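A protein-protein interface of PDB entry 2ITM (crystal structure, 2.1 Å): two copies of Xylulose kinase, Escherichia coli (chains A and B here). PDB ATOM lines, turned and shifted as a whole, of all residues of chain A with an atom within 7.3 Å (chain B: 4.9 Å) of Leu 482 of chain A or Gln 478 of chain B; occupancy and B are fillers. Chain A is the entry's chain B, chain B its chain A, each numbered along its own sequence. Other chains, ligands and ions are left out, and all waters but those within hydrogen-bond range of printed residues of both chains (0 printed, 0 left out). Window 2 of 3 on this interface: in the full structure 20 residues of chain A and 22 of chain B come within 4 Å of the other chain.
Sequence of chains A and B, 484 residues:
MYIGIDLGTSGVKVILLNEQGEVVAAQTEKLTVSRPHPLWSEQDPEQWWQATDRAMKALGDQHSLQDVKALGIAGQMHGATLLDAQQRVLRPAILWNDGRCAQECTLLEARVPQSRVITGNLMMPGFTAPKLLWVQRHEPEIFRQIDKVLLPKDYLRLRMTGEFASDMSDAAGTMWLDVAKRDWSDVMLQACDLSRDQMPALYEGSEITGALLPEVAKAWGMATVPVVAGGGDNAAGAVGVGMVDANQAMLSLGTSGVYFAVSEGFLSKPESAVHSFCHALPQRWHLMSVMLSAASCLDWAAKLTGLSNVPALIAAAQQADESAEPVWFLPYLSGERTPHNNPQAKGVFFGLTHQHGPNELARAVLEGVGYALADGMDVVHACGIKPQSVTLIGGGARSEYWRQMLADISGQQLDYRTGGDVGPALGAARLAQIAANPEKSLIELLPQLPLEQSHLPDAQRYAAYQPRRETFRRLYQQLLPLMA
Leu 479 of chain A touches Leu 479 of chain B.
CD2 of Leu 479 of chain A touches CD2 of Leu 482 of chain B (3.8 Å).
Leu 482 of chain A touches Phe 350 of chain B.
CD1 of Leu 482 of chain A touches OE1 of Gln 478 of chain B, 3.4 Å away.
Phe 350 of chain B touches Met 483 of chain A (CE1 to SD, 3.5 Å).
Of chain A, only Leu 482 (3.4 Å) comes within 4 Å of Gln 478 of chain B.
Of the printed residues of chain A, Leu 479 of chain B touches Leu 479 (3.7 Å).
Printed residues of chain A within 4 Å of Leu 482 of chain B: Leu 479 (3.8 Å).
Printed residues of chain B within 4 Å of Leu 479 of chain A: Leu 479 (3.7 Å) and Leu 482 (3.8 Å).
Printed residues of chain A within 4 Å of Phe 350 of chain B: Leu 482 (3.6 Å) and Met 483 (3.5 Å).
Of the printed residues of chain B, Met 483 of chain A touches Phe 350.
Gln 477 of chain B touches none of the printed residues of chain A.
The nearest printed residue of chain A that does not touch Leu 482 of chain B is Gln 478 of chain A (4.1 Å).
Hydrophobic or aromatic side chains of chain B that line the printed part of chain A: Phe 350, Leu 479 and Leu 482.
Along chain B the printed residues that touch a printed residue of chain A span positions 350 to 482.
Hydrophobic or aromatic side chains of chain A within 4 Å of the printed part of chain B: Leu 479, Leu 482 and Met 483.
Along chain A the printed residues that touch a printed residue of chain B span positions 479 to 483.
Among the printed residues, 5 pairs touch across the chains.
Among the printed residues, no Asp or Glu carboxylate lies within 4 Å of a Lys or Arg side-chain nitrogen of the other chain.
Leu 479 of chain A touches its own counterpart, Leu 479 of chain B.
Leu 479 of chain A touches Leu 482 of chain B, but with the chains exchanged Leu 482 of chain A does not touch Leu 479 of chain B (5.3 Å).
Leu 482 of chain A touches Gln 478 of chain B, but with the chains exchanged Gln 478 of chain A does not touch Leu 482 of chain B (4.1 Å).
6 positions are printed for both chains.
Of the 5 pairs that touch across the chains among the printed residues, 1 has its exchanged pair printed and touching as well.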
ATOM      1  N   TYR A 332      19.356 -19.202   1.615  1.00  0.00           N
ATOM      2  CA  TYR A 332      18.745 -19.118   0.313  1.00  0.00           C
ATOM      3  C   TYR A 332      18.872 -20.406  -0.431  1.00  0.00           C
ATOM      4  O   TYR A 332      19.890 -20.701  -0.975  1.00  0.00           O
ATOM      5  CB  TYR A 332      19.284 -17.970  -0.514  1.00  0.00           C
ATOM      6  CG  TYR A 332      18.892 -16.637   0.034  1.00  0.00           C
ATOM      7  CD1 TYR A 332      19.743 -15.929   0.864  1.00  0.00           C
ATOM      8  CD2 TYR A 332      17.663 -16.109  -0.241  1.00  0.00           C
ATOM      9  CE1 TYR A 332      19.390 -14.766   1.369  1.00  0.00           C
ATOM     10  CE2 TYR A 332      17.307 -14.950   0.264  1.00  0.00           C
ATOM     11  CZ  TYR A 332      18.161 -14.267   1.074  1.00  0.00           C
ATOM     12  OH  TYR A 332      17.764 -13.094   1.579  1.00  0.00           O
ATOM     13  N   VAL A 348      23.240 -15.331   4.422  1.00  0.00           N
ATOM     14  CA  VAL A 348      23.602 -14.058   5.013  1.00  0.00           C
ATOM     15  C   VAL A 348      23.498 -14.149   6.536  1.00  0.00           C
ATOM     16  O   VAL A 348      22.527 -14.670   7.063  1.00  0.00           O
ATOM     17  CB  VAL A 348      22.664 -12.916   4.502  1.00  0.00           C
ATOM     18  CG1 VAL A 348      22.919 -11.636   5.239  1.00  0.00           C
ATOM     19  CG2 VAL A 348      22.795 -12.709   3.007  1.00  0.00           C
ATOM     20  N   GLN A 477      13.261 -10.930   2.536  1.00  0.00           N
ATOM     21  CA  GLN A 477      12.624 -10.285   1.403  1.00  0.00           C
ATOM     22  C   GLN A 477      13.508  -9.200   0.809  1.00  0.00           C
ATOM     23  O   GLN A 477      13.645  -9.093  -0.393  1.00  0.00           O
ATOM     24  CB  GLN A 477      11.257  -9.722   1.805  1.00  0.00           C
ATOM     25  CG  GLN A 477      10.123 -10.745   1.776  1.00  0.00           C
ATOM     26  CD  GLN A 477       8.896 -10.330   2.588  1.00  0.00           C
ATOM     27  OE1 GLN A 477       8.848  -9.238   3.149  1.00  0.00           O
ATOM     28  NE2 GLN A 477       7.903 -11.215   2.646  1.00  0.00           N
ATOM     29  N   GLN A 478      14.105  -8.397   1.665  1.00  0.00           N
ATOM     30  CA  GLN A 478      14.915  -7.293   1.204  1.00  0.00           C
ATOM     31  C   GLN A 478      16.187  -7.718   0.474  1.00  0.00           C
ATOM     32  O   GLN A 478      16.555  -7.120  -0.523  1.00  0.00           O
ATOM     33  CB  GLN A 478      15.222  -6.332   2.345  1.00  0.00           C
ATOM     34  CG  GLN A 478      14.068  -5.428   2.693  1.00  0.00           C
ATOM     35  CD  GLN A 478      13.635  -4.577   1.543  1.00  0.00           C
ATOM     36  OE1 GLN A 478      14.397  -3.756   1.059  1.00  0.00           O
ATOM     37  NE2 GLN A 478      12.413  -4.769   1.097  1.00  0.00           N
ATOM     38  N   LEU A 479      16.839  -8.762   0.955  1.00  0.00           N
ATOM     39  CA  LEU A 479      18.095  -9.188   0.361  1.00  0.00           C
ATOM     40  C   LEU A 479      17.955 -10.203  -0.774  1.00  0.00           C
ATOM     41  O   LEU A 479      18.915 -10.484  -1.462  1.00  0.00           O
ATOM     42  CB  LEU A 479      19.060  -9.714   1.417  1.00  0.00           C
ATOM     43  CG  LEU A 479      19.182  -8.980   2.747  1.00  0.00           C
ATOM     44  CD1 LEU A 479      20.441  -9.369   3.444  1.00  0.00           C
ATOM     45  CD2 LEU A 479      19.134  -7.504   2.550  1.00  0.00           C
ATOM     46  N   LEU A 480      16.765 -10.760  -0.949  1.00  0.00           N
ATOM     47  CA  LEU A 480      16.545 -11.836  -1.935  1.00  0.00           C
ATOM     48  C   LEU A 480      17.046 -11.481  -3.327  1.00  0.00           C
ATOM     49  O   LEU A 480      17.800 -12.226  -3.917  1.00  0.00           O
ATOM     50  CB  LEU A 480      15.073 -12.247  -1.979  1.00  0.00           C
ATOM     51  CG  LEU A 480      14.630 -13.366  -2.930  1.00  0.00           C
ATOM     52  CD1 LEU A 480      14.817 -12.931  -4.362  1.00  0.00           C
ATOM     53  CD2 LEU A 480      15.363 -14.654  -2.665  1.00  0.00           C
ATOM     54  N   PRO A 481      16.652 -10.329  -3.830  1.00  0.00           N
ATOM     55  CA  PRO A 481      17.074  -9.907  -5.158  1.00  0.00           C
ATOM     56  C   PRO A 481      18.565  -9.650  -5.252  1.00  0.00           C
ATOM     57  O   PRO A 481      19.096  -9.574  -6.345  1.00  0.00           O
ATOM     58  CB  PRO A 481      16.291  -8.616  -5.375  1.00  0.00           C
ATOM     59  CG  PRO A 481      15.633  -8.324  -4.066  1.00  0.00           C
ATOM     60  CD  PRO A 481      15.457  -9.605  -3.381  1.00  0.00           C
ATOM     61  N   LEU A 482      19.232  -9.539  -4.114  1.00  0.00           N
ATOM     62  CA  LEU A 482      20.663  -9.357  -4.083  1.00  0.00           C
ATOM     63  C   LEU A 482      21.333 -10.713  -4.251  1.00  0.00           C
ATOM     64  O   LEU A 482      22.390 -10.825  -4.825  1.00  0.00           O
ATOM     65  CB  LEU A 482      21.101  -8.714  -2.773  1.00  0.00           C
ATOM     66  CG  LEU A 482      21.230  -7.202  -2.823  1.00  0.00           C
ATOM     67  CD1 LEU A 482      21.887  -6.851  -4.123  1.00  0.00           C
ATOM     68  CD2 LEU A 482      19.913  -6.560  -2.737  1.00  0.00           C
ATOM     69  N   MET A 483      20.691 -11.737  -3.720  1.00  0.00           N
ATOM     70  CA  MET A 483      21.226 -13.084  -3.712  1.00  0.00           C
ATOM     71  C   MET A 483      20.600 -13.898  -4.843  1.00  0.00           C
ATOM     72  O   MET A 483      20.090 -14.993  -4.632  1.00  0.00           O
ATOM     73  CB  MET A 483      20.978 -13.763  -2.363  1.00  0.00           C
ATOM     74  CG  MET A 483      21.558 -13.049  -1.155  1.00  0.00           C
ATOM     75  SD  MET A 483      23.340 -13.176  -0.931  1.00  0.00           S
ATOM     76  CE  MET A 483      23.501 -14.915  -0.581  1.00  0.00           C
ATOM     77  N   ALA A 484      20.642 -13.334  -6.044  1.00  0.00           N
ATOM     78  CA  ALA A 484      19.811 -13.756  -7.168  1.00  0.00           C
ATOM     79  C   ALA A 484      20.043 -12.820  -8.341  1.00  0.00           C
ATOM     80  O   ALA A 484      20.806 -13.128  -9.250  1.00  0.00           O
ATOM     81  CB  ALA A 484      18.356 -13.773  -6.787  1.00  0.00           C
ATOM     82  OXT ALA A 484      19.454 -11.847  -8.339  1.00  0.00           O
ATOM     83  N   PHE B 350      27.755 -11.120   3.701  1.00  0.00           N
ATOM     84  CA  PHE B 350      26.954 -11.204   2.497  1.00  0.00           C
ATOM     85  C   PHE B 350      27.564 -12.122   1.441  1.00  0.00           C
ATOM     86  O   PHE B 350      28.706 -11.992   1.091  1.00  0.00           O
ATOM     87  CB  PHE B 350      26.749  -9.812   1.908  1.00  0.00           C
ATOM     88  CG  PHE B 350      25.877  -9.796   0.706  1.00  0.00           C
ATOM     89  CD1 PHE B 350      24.507  -9.779   0.833  1.00  0.00           C
ATOM     90  CD2 PHE B 350      26.421  -9.816  -0.549  1.00  0.00           C
ATOM     91  CE1 PHE B 350      23.712  -9.777  -0.258  1.00  0.00           C
ATOM     92  CE2 PHE B 350      25.627  -9.818  -1.646  1.00  0.00           C
ATOM     93  CZ  PHE B 350      24.266  -9.799  -1.500  1.00  0.00           C
ATOM     94  N   ARG B 474      28.759   0.067  -3.095  1.00  0.00           N
ATOM     95  CA  ARG B 474      27.440  -0.223  -3.636  1.00  0.00           C
ATOM     96  C   ARG B 474      26.611  -1.031  -2.654  1.00  0.00           C
ATOM     97  O   ARG B 474      25.511  -0.657  -2.305  1.00  0.00           O
ATOM     98  CB  ARG B 474      27.580  -1.003  -4.944  1.00  0.00           C
ATOM     99  CG  ARG B 474      26.421  -0.886  -5.909  1.00  0.00           C
ATOM    100  CD  ARG B 474      26.067  -2.174  -6.657  1.00  0.00           C
ATOM    101  NE  ARG B 474      27.228  -2.901  -7.157  1.00  0.00           N
ATOM    102  CZ  ARG B 474      28.214  -2.356  -7.849  1.00  0.00           C
ATOM    103  NH1 ARG B 474      28.194  -1.063  -8.136  1.00  0.00           N
ATOM    104  NH2 ARG B 474      29.210  -3.095  -8.253  1.00  0.00           N
ATOM    105  N   LEU B 475      27.167  -2.145  -2.208  1.00  0.00           N
ATOM    106  CA  LEU B 475      26.505  -3.001  -1.253  1.00  0.00           C
ATOM    107  C   LEU B 475      26.247  -2.305   0.078  1.00  0.00           C
ATOM    108  O   LEU B 475      25.166  -2.409   0.622  1.00  0.00           O
ATOM    109  CB  LEU B 475      27.303  -4.282  -1.038  1.00  0.00           C
ATOM    110  CG  LEU B 475      27.368  -5.360  -2.120  1.00  0.00           C
ATOM    111  CD1 LEU B 475      28.164  -6.543  -1.649  1.00  0.00           C
ATOM    112  CD2 LEU B 475      25.997  -5.798  -2.560  1.00  0.00           C
ATOM    113  N   TYR B 476      27.248  -1.607   0.598  1.00  0.00           N
ATOM    114  CA  TYR B 476      27.130  -0.911   1.876  1.00  0.00           C
ATOM    115  C   TYR B 476      25.953   0.064   1.850  1.00  0.00           C
ATOM    116  O   TYR B 476      25.075   0.023   2.690  1.00  0.00           O
ATOM    117  CB  TYR B 476      28.439  -0.183   2.188  1.00  0.00           C
ATOM    118  CG  TYR B 476      28.518   0.528   3.521  1.00  0.00           C
ATOM    119  CD1 TYR B 476      29.087  -0.079   4.625  1.00  0.00           C
ATOM    120  CD2 TYR B 476      28.063   1.822   3.663  1.00  0.00           C
ATOM    121  CE1 TYR B 476      29.169   0.569   5.829  1.00  0.00           C
ATOM    122  CE2 TYR B 476      28.145   2.468   4.859  1.00  0.00           C
ATOM    123  CZ  TYR B 476      28.696   1.840   5.941  1.00  0.00           C
ATOM    124  OH  TYR B 476      28.777   2.492   7.132  1.00  0.00           O
ATOM    125  N   GLN B 477      25.933   0.923   0.847  1.00  0.00           N
ATOM    126  CA  GLN B 477      24.794   1.778   0.627  1.00  0.00           C
ATOM    127  C   GLN B 477      23.446   1.057   0.584  1.00  0.00           C
ATOM    128  O   GLN B 477      22.504   1.476   1.225  1.00  0.00           O
ATOM    129  CB  GLN B 477      25.010   2.645  -0.594  1.00  0.00           C
ATOM    130  CG  GLN B 477      25.945   3.814  -0.346  1.00  0.00           C
ATOM    131  CD  GLN B 477      25.515   4.669   0.831  1.00  0.00           C
ATOM    132  OE1 GLN B 477      24.402   5.183   0.849  1.00  0.00           O
ATOM    133  NE2 GLN B 477      26.398   4.820   1.816  1.00  0.00           N
ATOM    134  N   GLN B 478      23.376  -0.041  -0.150  1.00  0.00           N
ATOM    135  CA  GLN B 478      22.139  -0.787  -0.299  1.00  0.00           C
ATOM    136  C   GLN B 478      21.507  -1.238   1.017  1.00  0.00           C
ATOM    137  O   GLN B 478      20.303  -1.171   1.170  1.00  0.00           O
ATOM    138  CB  GLN B 478      22.341  -1.981  -1.224  1.00  0.00           C
ATOM    139  CG  GLN B 478      22.111  -1.689  -2.687  1.00  0.00           C
ATOM    140  CD  GLN B 478      21.985  -2.949  -3.505  1.00  0.00           C
ATOM    141  OE1 GLN B 478      22.963  -3.629  -3.746  1.00  0.00           O
ATOM    142  NE2 GLN B 478      20.778  -3.267  -3.914  1.00  0.00           N
ATOM    143  N   LEU B 479      22.332  -1.687   1.956  1.00  0.00           N
ATOM    144  CA  LEU B 479      21.856  -2.255   3.212  1.00  0.00           C
ATOM    145  C   LEU B 479      21.802  -1.217   4.327  1.00  0.00           C
ATOM    146  O   LEU B 479      21.325  -1.488   5.411  1.00  0.00           O
ATOM    147  CB  LEU B 479      22.742  -3.423   3.644  1.00  0.00           C
ATOM    148  CG  LEU B 479      22.873  -4.639   2.733  1.00  0.00           C
ATOM    149  CD1 LEU B 479      23.188  -5.873   3.522  1.00  0.00           C
ATOM    150  CD2 LEU B 479      21.611  -4.851   1.944  1.00  0.00           C
ATOM    151  N   LEU B 480      22.315  -0.033   4.037  1.00  0.00           N
ATOM    152  CA  LEU B 480      22.441   1.041   5.005  1.00  0.00           C
ATOM    153  C   LEU B 480      21.133   1.365   5.728  1.00  0.00           C
ATOM    154  O   LEU B 480      21.120   1.560   6.926  1.00  0.00           O
ATOM    155  CB  LEU B 480      22.960   2.293   4.312  1.00  0.00           C
ATOM    156  CG  LEU B 480      23.829   3.276   5.077  1.00  0.00           C
ATOM    157  CD1 LEU B 480      23.769   4.644   4.451  1.00  0.00           C
ATOM    158  CD2 LEU B 480      23.474   3.338   6.514  1.00  0.00           C
ATOM    159  N   PRO B 481      20.042   1.432   4.987  1.00  0.00           N
ATOM    160  CA  PRO B 481      18.749   1.773   5.575  1.00  0.00           C
ATOM    161  C   PRO B 481      18.264   0.683   6.512  1.00  0.00           C
ATOM    162  O   PRO B 481      17.549   0.954   7.451  1.00  0.00           O
ATOM    163  CB  PRO B 481      17.842   1.867   4.363  1.00  0.00           C
ATOM    164  CG  PRO B 481      18.721   2.149   3.286  1.00  0.00           C
ATOM    165  CD  PRO B 481      19.979   1.425   3.525  1.00  0.00           C
ATOM    166  N   LEU B 482      18.683  -0.540   6.246  1.00  0.00           N
ATOM    167  CA  LEU B 482      18.372  -1.679   7.082  1.00  0.00           C
ATOM    168  C   LEU B 482      19.109  -1.653   8.413  1.00  0.00           C
ATOM    169  O   LEU B 482      18.702  -2.318   9.350  1.00  0.00           O
ATOM    170  CB  LEU B 482      18.696  -2.963   6.334  1.00  0.00           C
ATOM    171  CG  LEU B 482      17.616  -3.662   5.517  1.00  0.00           C
ATOM    172  CD1 LEU B 482      16.464  -2.773   5.162  1.00  0.00           C
ATOM    173  CD2 LEU B 482      18.210  -4.276   4.290  1.00  0.00           C
